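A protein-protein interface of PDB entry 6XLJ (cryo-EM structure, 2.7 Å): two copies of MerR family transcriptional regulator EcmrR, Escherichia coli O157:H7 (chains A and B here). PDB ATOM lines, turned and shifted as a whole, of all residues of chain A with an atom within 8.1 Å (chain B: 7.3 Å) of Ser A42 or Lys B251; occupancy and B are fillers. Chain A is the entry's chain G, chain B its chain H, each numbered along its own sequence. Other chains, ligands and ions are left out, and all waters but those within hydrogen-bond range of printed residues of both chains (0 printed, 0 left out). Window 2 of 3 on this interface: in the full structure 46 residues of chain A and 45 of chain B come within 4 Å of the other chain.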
ATOM      1  N   SER A   1     -12.619 -25.392 -36.795  1.00  0.00           N
ATOM      2  CA  SER A   1     -11.427 -25.845 -36.091  1.00  0.00           C
ATOM      3  C   SER A   1     -10.982 -27.179 -36.631  1.00  0.00           C
ATOM      4  O   SER A   1     -11.657 -28.182 -36.448  1.00  0.00           O
ATOM      5  CB  SER A   1     -11.683 -25.958 -34.594  1.00  0.00           C
ATOM      6  OG  SER A   1     -12.741 -26.866 -34.345  1.00  0.00           O
ATOM      7  N   PHE A   6      -8.138 -28.413 -32.808  1.00  0.00           N
ATOM      8  CA  PHE A   6      -9.103 -28.888 -31.828  1.00  0.00           C
ATOM      9  C   PHE A   6      -8.459 -29.864 -30.858  1.00  0.00           C
ATOM     10  O   PHE A   6      -8.768 -29.854 -29.663  1.00  0.00           O
ATOM     11  CB  PHE A   6     -10.279 -29.533 -32.545  1.00  0.00           C
ATOM     12  CG  PHE A   6     -11.369 -29.946 -31.640  1.00  0.00           C
ATOM     13  CD1 PHE A   6     -12.274 -29.020 -31.189  1.00  0.00           C
ATOM     14  CD2 PHE A   6     -11.504 -31.249 -31.240  1.00  0.00           C
ATOM     15  CE1 PHE A   6     -13.290 -29.383 -30.350  1.00  0.00           C
ATOM     16  CE2 PHE A   6     -12.523 -31.619 -30.398  1.00  0.00           C
ATOM     17  CZ  PHE A   6     -13.417 -30.685 -29.955  1.00  0.00           C
ATOM     18  N   ILE A   9      -6.852 -27.793 -28.434  1.00  0.00           N
ATOM     19  CA  ILE A   9      -7.838 -27.162 -27.558  1.00  0.00           C
ATOM     20  C   ILE A   9      -8.205 -28.097 -26.419  1.00  0.00           C
ATOM     21  O   ILE A   9      -8.048 -27.767 -25.239  1.00  0.00           O
ATOM     22  CB  ILE A   9      -9.084 -26.734 -28.350  1.00  0.00           C
ATOM     23  CG1 ILE A   9      -8.786 -25.486 -29.169  1.00  0.00           C
ATOM     24  CG2 ILE A   9     -10.264 -26.504 -27.427  1.00  0.00           C
ATOM     25  CD1 ILE A   9      -9.953 -25.027 -30.003  1.00  0.00           C
ATOM     26  N   ALA A  29     -18.415 -32.087 -36.486  1.00  0.00           N
ATOM     27  CA  ALA A  29     -19.584 -31.418 -37.029  1.00  0.00           C
ATOM     28  C   ALA A  29     -19.611 -31.505 -38.544  1.00  0.00           C
ATOM     29  O   ALA A  29     -20.681 -31.667 -39.139  1.00  0.00           O
ATOM     30  CB  ALA A  29     -19.601 -29.964 -36.573  1.00  0.00           C
ATOM     31  N   PHE A  39     -13.489 -31.389 -39.250  1.00  0.00           N
ATOM     32  CA  PHE A  39     -13.554 -30.064 -38.654  1.00  0.00           C
ATOM     33  C   PHE A  39     -14.599 -30.052 -37.557  1.00  0.00           C
ATOM     34  O   PHE A  39     -15.725 -30.515 -37.757  1.00  0.00           O
ATOM     35  CB  PHE A  39     -13.914 -28.971 -39.661  1.00  0.00           C
ATOM     36  CG  PHE A  39     -13.040 -28.921 -40.866  1.00  0.00           C
ATOM     37  CD1 PHE A  39     -11.870 -28.199 -40.848  1.00  0.00           C
ATOM     38  CD2 PHE A  39     -13.409 -29.553 -42.029  1.00  0.00           C
ATOM     39  CE1 PHE A  39     -11.072 -28.133 -41.956  1.00  0.00           C
ATOM     40  CE2 PHE A  39     -12.611 -29.490 -43.142  1.00  0.00           C
ATOM     41  CZ  PHE A  39     -11.440 -28.781 -43.101  1.00  0.00           C
ATOM     42  N   TYR A  40     -14.217 -29.537 -36.402  1.00  0.00           N
ATOM     43  CA  TYR A  40     -15.078 -29.503 -35.239  1.00  0.00           C
ATOM     44  C   TYR A  40     -15.508 -28.069 -34.990  1.00  0.00           C
ATOM     45  O   TYR A  40     -15.011 -27.124 -35.602  1.00  0.00           O
ATOM     46  CB  TYR A  40     -14.384 -30.066 -34.001  1.00  0.00           C
ATOM     47  CG  TYR A  40     -13.899 -31.471 -34.160  1.00  0.00           C
ATOM     48  CD1 TYR A  40     -12.678 -31.748 -34.733  1.00  0.00           C
ATOM     49  CD2 TYR A  40     -14.683 -32.528 -33.752  1.00  0.00           C
ATOM     50  CE1 TYR A  40     -12.247 -33.035 -34.875  1.00  0.00           C
ATOM     51  CE2 TYR A  40     -14.261 -33.811 -33.890  1.00  0.00           C
ATOM     52  CZ  TYR A  40     -13.049 -34.062 -34.455  1.00  0.00           C
ATOM     53  OH  TYR A  40     -12.636 -35.360 -34.591  1.00  0.00           O
ATOM     54  N   THR A  41     -16.429 -27.920 -34.052  1.00  0.00           N
ATOM     55  CA  THR A  41     -16.949 -26.629 -33.652  1.00  0.00           C
ATOM     56  C   THR A  41     -16.902 -26.559 -32.131  1.00  0.00           C
ATOM     57  O   THR A  41     -16.422 -27.476 -31.464  1.00  0.00           O
ATOM     58  CB  THR A  41     -18.364 -26.431 -34.204  1.00  0.00           C
ATOM     59  OG1 THR A  41     -18.319 -26.478 -35.633  1.00  0.00           O
ATOM     60  CG2 THR A  41     -18.925 -25.081 -33.804  1.00  0.00           C
ATOM     61  N   SER A  42     -17.364 -25.440 -31.577  1.00  0.00           N
ATOM     62  CA  SER A  42     -17.426 -25.296 -30.130  1.00  0.00           C
ATOM     63  C   SER A  42     -18.334 -26.346 -29.501  1.00  0.00           C
ATOM     64  O   SER A  42     -18.032 -26.870 -28.423  1.00  0.00           O
ATOM     65  CB  SER A  42     -17.891 -23.888 -29.778  1.00  0.00           C
ATOM     66  OG  SER A  42     -19.301 -23.810 -29.800  1.00  0.00           O
ATOM     67  N   ASP A  43     -19.447 -26.680 -30.158  1.00  0.00           N
ATOM     68  CA  ASP A  43     -20.344 -27.684 -29.598  1.00  0.00           C
ATOM     69  C   ASP A  43     -19.821 -29.109 -29.752  1.00  0.00           C
ATOM     70  O   ASP A  43     -20.548 -30.053 -29.423  1.00  0.00           O
ATOM     71  CB  ASP A  43     -21.728 -27.569 -30.230  1.00  0.00           C
ATOM     72  CG  ASP A  43     -21.663 -27.338 -31.704  1.00  0.00           C
ATOM     73  OD1 ASP A  43     -20.557 -27.464 -32.249  1.00  0.00           O
ATOM     74  OD2 ASP A  43     -22.703 -27.041 -32.320  1.00  0.00           O
ATOM     75  N   GLN A  44     -18.606 -29.295 -30.266  1.00  0.00           N
ATOM     76  CA  GLN A  44     -17.884 -30.552 -30.103  1.00  0.00           C
ATOM     77  C   GLN A  44     -16.968 -30.509 -28.899  1.00  0.00           C
ATOM     78  O   GLN A  44     -16.768 -31.534 -28.245  1.00  0.00           O
ATOM     79  CB  GLN A  44     -17.080 -30.909 -31.351  1.00  0.00           C
ATOM     80  CG  GLN A  44     -17.843 -30.707 -32.612  1.00  0.00           C
ATOM     81  CD  GLN A  44     -19.182 -31.393 -32.559  1.00  0.00           C
ATOM     82  OE1 GLN A  44     -20.219 -30.744 -32.478  1.00  0.00           O
ATOM     83  NE2 GLN A  44     -19.169 -32.713 -32.578  1.00  0.00           N
ATOM     84  N   LEU A  45     -16.424 -29.340 -28.581  1.00  0.00           N
ATOM     85  CA  LEU A  45     -15.674 -29.206 -27.344  1.00  0.00           C
ATOM     86  C   LEU A  45     -16.601 -29.337 -26.150  1.00  0.00           C
ATOM     87  O   LEU A  45     -16.227 -29.913 -25.120  1.00  0.00           O
ATOM     88  CB  LEU A  45     -14.962 -27.862 -27.314  1.00  0.00           C
ATOM     89  CG  LEU A  45     -14.389 -27.398 -25.981  1.00  0.00           C
ATOM     90  CD1 LEU A  45     -13.308 -28.331 -25.505  1.00  0.00           C
ATOM     91  CD2 LEU A  45     -13.855 -25.999 -26.131  1.00  0.00           C
ATOM     92  N   MET A  46     -17.815 -28.803 -26.270  1.00  0.00           N
ATOM     93  CA  MET A  46     -18.804 -28.962 -25.211  1.00  0.00           C
ATOM     94  C   MET A  46     -19.121 -30.425 -24.937  1.00  0.00           C
ATOM     95  O   MET A  46     -19.360 -30.799 -23.785  1.00  0.00           O
ATOM     96  CB  MET A  46     -20.077 -28.197 -25.574  1.00  0.00           C
ATOM     97  CG  MET A  46     -21.234 -28.286 -24.574  1.00  0.00           C
ATOM     98  SD  MET A  46     -22.292 -29.740 -24.772  1.00  0.00           S
ATOM     99  CE  MET A  46     -22.998 -29.436 -26.384  1.00  0.00           C
ATOM    100  N   LYS A  47     -19.084 -31.275 -25.959  1.00  0.00           N
ATOM    101  CA  LYS A  47     -19.340 -32.686 -25.716  1.00  0.00           C
ATOM    102  C   LYS A  47     -18.087 -33.421 -25.264  1.00  0.00           C
ATOM    103  O   LYS A  47     -18.174 -34.347 -24.448  1.00  0.00           O
ATOM    104  CB  LYS A  47     -19.933 -33.322 -26.969  1.00  0.00           C
ATOM    105  CG  LYS A  47     -20.455 -34.720 -26.774  1.00  0.00           C
ATOM    106  CD  LYS A  47     -20.918 -35.311 -28.090  1.00  0.00           C
ATOM    107  CE  LYS A  47     -21.452 -36.720 -27.894  1.00  0.00           C
ATOM    108  NZ  LYS A  47     -21.772 -37.399 -29.179  1.00  0.00           N
ATOM    109  N   PHE A  48     -16.920 -33.052 -25.795  1.00  0.00           N
ATOM    110  CA  PHE A  48     -15.688 -33.673 -25.328  1.00  0.00           C
ATOM    111  C   PHE A  48     -15.434 -33.391 -23.860  1.00  0.00           C
ATOM    112  O   PHE A  48     -14.854 -34.231 -23.165  1.00  0.00           O
ATOM    113  CB  PHE A  48     -14.482 -33.208 -26.135  1.00  0.00           C
ATOM    114  CG  PHE A  48     -13.196 -33.855 -25.707  1.00  0.00           C
ATOM    115  CD1 PHE A  48     -12.783 -35.032 -26.292  1.00  0.00           C
ATOM    116  CD2 PHE A  48     -12.397 -33.296 -24.725  1.00  0.00           C
ATOM    117  CE1 PHE A  48     -11.608 -35.641 -25.901  1.00  0.00           C
ATOM    118  CE2 PHE A  48     -11.231 -33.908 -24.327  1.00  0.00           C
ATOM    119  CZ  PHE A  48     -10.834 -35.077 -24.917  1.00  0.00           C
ATOM    120  N   HIS A  49     -15.836 -32.222 -23.369  1.00  0.00           N
ATOM    121  CA  HIS A  49     -15.669 -31.960 -21.946  1.00  0.00           C
ATOM    122  C   HIS A  49     -16.484 -32.933 -21.110  1.00  0.00           C
ATOM    123  O   HIS A  49     -15.988 -33.480 -20.119  1.00  0.00           O
ATOM    124  CB  HIS A  49     -16.046 -30.520 -21.634  1.00  0.00           C
ATOM    125  CG  HIS A  49     -15.559 -30.055 -20.303  1.00  0.00           C
ATOM    126  ND1 HIS A  49     -16.320 -30.143 -19.160  1.00  0.00           N
ATOM    127  CD2 HIS A  49     -14.374 -29.521 -19.927  1.00  0.00           C
ATOM    128  CE1 HIS A  49     -15.631 -29.668 -18.140  1.00  0.00           C
ATOM    129  NE2 HIS A  49     -14.447 -29.284 -18.579  1.00  0.00           N
ATOM    130  N   ILE B 210     -17.816 -26.022 -18.000  1.00  0.00           N
ATOM    131  CA  ILE B 210     -18.195 -25.223 -19.164  1.00  0.00           C
ATOM    132  C   ILE B 210     -19.621 -24.694 -19.012  1.00  0.00           C
ATOM    133  O   ILE B 210     -20.582 -25.460 -18.879  1.00  0.00           O
ATOM    134  CB  ILE B 210     -18.024 -26.008 -20.477  1.00  0.00           C
ATOM    135  CG1 ILE B 210     -18.834 -27.305 -20.485  1.00  0.00           C
ATOM    136  CG2 ILE B 210     -16.552 -26.291 -20.729  1.00  0.00           C
ATOM    137  CD1 ILE B 210     -18.690 -28.087 -21.738  1.00  0.00           C
ATOM    138  N   ILE B 245     -14.120 -18.593 -24.437  1.00  0.00           N
ATOM    139  CA  ILE B 245     -13.831 -19.307 -25.667  1.00  0.00           C
ATOM    140  C   ILE B 245     -14.751 -18.872 -26.804  1.00  0.00           C
ATOM    141  O   ILE B 245     -14.284 -18.531 -27.891  1.00  0.00           O
ATOM    142  CB  ILE B 245     -13.849 -20.837 -25.444  1.00  0.00           C
ATOM    143  CG1 ILE B 245     -15.065 -21.290 -24.644  1.00  0.00           C
ATOM    144  CG2 ILE B 245     -12.575 -21.279 -24.747  1.00  0.00           C
ATOM    145  CD1 ILE B 245     -15.225 -22.785 -24.588  1.00  0.00           C
ATOM    146  N   ASP B 246     -16.060 -18.883 -26.577  1.00  0.00           N
ATOM    147  CA  ASP B 246     -17.019 -18.450 -27.581  1.00  0.00           C
ATOM    148  C   ASP B 246     -17.971 -17.436 -26.964  1.00  0.00           C
ATOM    149  O   ASP B 246     -18.350 -17.561 -25.797  1.00  0.00           O
ATOM    150  CB  ASP B 246     -17.740 -19.712 -28.103  1.00  0.00           C
ATOM    151  CG  ASP B 246     -18.826 -19.438 -29.127  1.00  0.00           C
ATOM    152  OD1 ASP B 246     -19.644 -18.505 -28.985  1.00  0.00           O
ATOM    153  OD2 ASP B 246     -18.843 -20.200 -30.115  1.00  0.00           O
ATOM    154  N   GLY B 247     -18.369 -16.438 -27.754  1.00  0.00           N
ATOM    155  CA  GLY B 247     -19.275 -15.430 -27.232  1.00  0.00           C
ATOM    156  C   GLY B 247     -19.829 -14.394 -28.194  1.00  0.00           C
ATOM    157  O   GLY B 247     -19.984 -14.634 -29.393  1.00  0.00           O
ATOM    158  N   ILE B 248     -20.117 -13.213 -27.643  1.00  0.00           N
ATOM    159  CA  ILE B 248     -20.718 -12.100 -28.376  1.00  0.00           C
ATOM    160  C   ILE B 248     -19.821 -11.570 -29.496  1.00  0.00           C
ATOM    161  O   ILE B 248     -20.307 -10.909 -30.419  1.00  0.00           O
ATOM    162  CB  ILE B 248     -21.126 -10.989 -27.385  1.00  0.00           C
ATOM    163  CG1 ILE B 248     -22.177 -10.073 -28.021  1.00  0.00           C
ATOM    164  CG2 ILE B 248     -19.908 -10.215 -26.905  1.00  0.00           C
ATOM    165  CD1 ILE B 248     -22.811  -9.111 -27.057  1.00  0.00           C
ATOM    166  N   TRP B 249     -18.524 -11.865 -29.455  1.00  0.00           N
ATOM    167  CA  TRP B 249     -17.648 -11.437 -30.539  1.00  0.00           C
ATOM    168  C   TRP B 249     -17.667 -12.407 -31.709  1.00  0.00           C
ATOM    169  O   TRP B 249     -17.418 -11.988 -32.844  1.00  0.00           O
ATOM    170  CB  TRP B 249     -16.232 -11.244 -30.016  1.00  0.00           C
ATOM    171  CG  TRP B 249     -15.622 -12.521 -29.623  1.00  0.00           C
ATOM    172  CD1 TRP B 249     -14.789 -13.308 -30.353  1.00  0.00           C
ATOM    173  CD2 TRP B 249     -15.761 -13.149 -28.350  1.00  0.00           C
ATOM    174  NE1 TRP B 249     -14.427 -14.411 -29.621  1.00  0.00           N
ATOM    175  CE2 TRP B 249     -15.006 -14.329 -28.382  1.00  0.00           C
ATOM    176  CE3 TRP B 249     -16.461 -12.827 -27.185  1.00  0.00           C
ATOM    177  CZ2 TRP B 249     -14.933 -15.192 -27.296  1.00  0.00           C
ATOM    178  CZ3 TRP B 249     -16.385 -13.679 -26.111  1.00  0.00           C
ATOM    179  CH2 TRP B 249     -15.625 -14.848 -26.170  1.00  0.00           C
ATOM    180  N   ASN B 250     -17.928 -13.689 -31.478  1.00  0.00           N
ATOM    181  CA  ASN B 250     -17.809 -14.653 -32.562  1.00  0.00           C
ATOM    182  C   ASN B 250     -19.181 -15.032 -33.097  1.00  0.00           C
ATOM    183  O   ASN B 250     -19.319 -15.288 -34.296  1.00  0.00           O
ATOM    184  CB  ASN B 250     -17.014 -15.898 -32.150  1.00  0.00           C
ATOM    185  CG  ASN B 250     -17.788 -16.829 -31.272  1.00  0.00           C
ATOM    186  OD1 ASN B 250     -18.134 -16.493 -30.146  1.00  0.00           O
ATOM    187  ND2 ASN B 250     -18.093 -18.010 -31.794  1.00  0.00           N
ATOM    188  N   LYS B 251     -20.192 -15.083 -32.229  1.00  0.00           N
ATOM    189  CA  LYS B 251     -21.559 -15.388 -32.633  1.00  0.00           C
ATOM    190  C   LYS B 251     -22.462 -14.486 -31.812  1.00  0.00           C
ATOM    191  O   LYS B 251     -22.446 -14.538 -30.579  1.00  0.00           O
ATOM    192  CB  LYS B 251     -21.951 -16.852 -32.416  1.00  0.00           C
ATOM    193  CG  LYS B 251     -21.238 -17.849 -33.297  1.00  0.00           C
ATOM    194  CD  LYS B 251     -21.555 -19.277 -32.875  1.00  0.00           C
ATOM    195  CE  LYS B 251     -21.562 -19.429 -31.372  1.00  0.00           C
ATOM    196  NZ  LYS B 251     -21.637 -20.846 -30.928  1.00  0.00           N
ATOM    197  N   GLN B 252     -23.268 -13.689 -32.500  1.00  0.00           N
ATOM    198  CA  GLN B 252     -24.096 -12.659 -31.887  1.00  0.00           C
ATOM    199  C   GLN B 252     -25.341 -13.200 -31.203  1.00  0.00           C
ATOM    200  O   GLN B 252     -26.115 -12.404 -30.662  1.00  0.00           O
ATOM    201  CB  GLN B 252     -24.466 -11.583 -32.912  1.00  0.00           C
ATOM    202  CG  GLN B 252     -23.287 -10.704 -33.367  1.00  0.00           C
ATOM    203  CD  GLN B 252     -22.237 -11.433 -34.183  1.00  0.00           C
ATOM    204  OE1 GLN B 252     -21.074 -11.512 -33.785  1.00  0.00           O
ATOM    205  NE2 GLN B 252     -22.641 -11.971 -35.329  1.00  0.00           N
ATOM    206  N   ASP B 253     -25.562 -14.510 -31.200  1.00  0.00           N
ATOM    207  CA  ASP B 253     -26.662 -15.074 -30.431  1.00  0.00           C
ATOM    208  C   ASP B 253     -26.165 -15.337 -29.016  1.00  0.00           C
ATOM    209  O   ASP B 253     -25.153 -16.014 -28.813  1.00  0.00           O
ATOM    210  CB  ASP B 253     -27.188 -16.353 -31.083  1.00  0.00           C
ATOM    211  CG  ASP B 253     -28.410 -16.907 -30.377  1.00  0.00           C
ATOM    212  OD1 ASP B 253     -29.507 -16.332 -30.552  1.00  0.00           O
ATOM    213  OD2 ASP B 253     -28.279 -17.910 -29.647  1.00  0.00           O
ATOM    214  N   SER B 254     -26.899 -14.800 -28.041  1.00  0.00           N
ATOM    215  CA  SER B 254     -26.516 -14.874 -26.639  1.00  0.00           C
ATOM    216  C   SER B 254     -26.602 -16.276 -26.065  1.00  0.00           C
ATOM    217  O   SER B 254     -25.963 -16.548 -25.043  1.00  0.00           O
ATOM    218  CB  SER B 254     -27.365 -13.921 -25.806  1.00  0.00           C
ATOM    219  OG  SER B 254     -26.771 -13.712 -24.535  1.00  0.00           O
ATOM    220  N   ALA B 255     -27.367 -17.168 -26.673  1.00  0.00           N
ATOM    221  CA  ALA B 255     -27.550 -18.482 -26.084  1.00  0.00           C
ATOM    222  C   ALA B 255     -26.543 -19.499 -26.592  1.00  0.00           C
ATOM    223  O   ALA B 255     -26.607 -20.663 -26.192  1.00  0.00           O
ATOM    224  CB  ALA B 255     -28.972 -18.985 -26.346  1.00  0.00           C
ATOM    225  N   GLU B 256     -25.623 -19.097 -27.468  1.00  0.00           N
ATOM    226  CA  GLU B 256     -24.585 -19.995 -27.951  1.00  0.00           C
ATOM    227  C   GLU B 256     -23.213 -19.644 -27.380  1.00  0.00           C
ATOM    228  O   GLU B 256     -22.187 -20.013 -27.956  1.00  0.00           O
ATOM    229  CB  GLU B 256     -24.563 -20.010 -29.474  1.00  0.00           C
ATOM    230  CG  GLU B 256     -25.461 -21.095 -30.023  1.00  0.00           C
ATOM    231  CD  GLU B 256     -25.036 -22.480 -29.580  1.00  0.00           C
ATOM    232  OE1 GLU B 256     -23.817 -22.737 -29.500  1.00  0.00           O
ATOM    233  OE2 GLU B 256     -25.927 -23.303 -29.284  1.00  0.00           O
ATOM    234  N   TRP B 257     -23.190 -18.880 -26.296  1.00  0.00           N
ATOM    235  CA  TRP B 257     -21.962 -18.472 -25.626  1.00  0.00           C
ATOM    236  C   TRP B 257     -21.366 -19.613 -24.814  1.00  0.00           C
ATOM    237  O   TRP B 257     -22.092 -20.419 -24.226  1.00  0.00           O
ATOM    238  CB  TRP B 257     -22.237 -17.270 -24.732  1.00  0.00           C
ATOM    239  CG  TRP B 257     -22.633 -16.041 -25.483  1.00  0.00           C
ATOM    240  CD1 TRP B 257     -22.814 -15.915 -26.829  1.00  0.00           C
ATOM    241  CD2 TRP B 257     -23.006 -14.787 -24.913  1.00  0.00           C
ATOM    242  NE1 TRP B 257     -23.210 -14.639 -27.137  1.00  0.00           N
ATOM    243  CE2 TRP B 257     -23.340 -13.930 -25.974  1.00  0.00           C
ATOM    244  CE3 TRP B 257     -23.065 -14.298 -23.606  1.00  0.00           C
ATOM    245  CZ2 TRP B 257     -23.743 -12.623 -25.770  1.00  0.00           C
ATOM    246  CZ3 TRP B 257     -23.450 -12.999 -23.406  1.00  0.00           C
ATOM    247  CH2 TRP B 257     -23.784 -12.172 -24.483  1.00  0.00           C
ATOM    248  N   MET B 258     -20.035 -19.662 -24.767  1.00  0.00           N
ATOM    249  CA  MET B 258     -19.307 -20.736 -24.102  1.00  0.00           C
ATOM    250  C   MET B 258     -18.220 -20.142 -23.217  1.00  0.00           C
ATOM    251  O   MET B 258     -17.383 -19.383 -23.712  1.00  0.00           O
ATOM    252  CB  MET B 258     -18.607 -21.646 -25.119  1.00  0.00           C
ATOM    253  CG  MET B 258     -19.378 -22.349 -26.214  1.00  0.00           C
ATOM    254  SD  MET B 258     -20.586 -23.581 -25.741  1.00  0.00           S
ATOM    255  CE  MET B 258     -22.040 -22.792 -26.390  1.00  0.00           C
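No position is printed for both chains.
Ser A42 touches just these residues of chain B: Asp B246, Lys B251 and Met B258. Of the printed residues of chain B, Leu A45 touches Ile B245. Lys A47 touches none of the printed residues of chain B. Of the printed residues of chain A, Ile B210 touches Met A46 (3.5 Å) and His A49 (3.6 Å). Gly B247 touches none of the printed residues of chain A. No residue of chain A comes within 4 Å of Asn B250. Lys B251 touches just one residue of chain A: Ser A42. The nearest residue of chain B that does not touch Ser A42 is Glu B256 (4.7 Å).
N of Ile B245 sits close to O of Met B258, at 3.4 Å. OD1 of Asp B246 lies close to OD1 of Asn B250 (2.8 Å). OD2 of Asp B246 is in salt-bridge range of NZ of Lys B251 (3.0 Å). The backbone carbonyl oxygen (O) of Asp B246 is in hydrogen-bond range of the backbone NH (N) of Met B258. NZ of Lys B251 is in salt-bridge range of OE1 of Glu B256 (3.2 Å).
Of the 15 printed residues of chain B, 5 touch a printed residue of chain A. Hydrophobic or aromatic side chains of chain B within 4 Å of the printed part of chain A: Ile B210, Ile B245 and Met B258.
Among the printed residues, merely in contact across the chains: Met A46 with Ile B210, His A49 with Ile B210, Ser A42 with Asp B246, Leu A45 with Ile B245, Ser A42 with Met B258 and Ser A42 with Lys B251.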
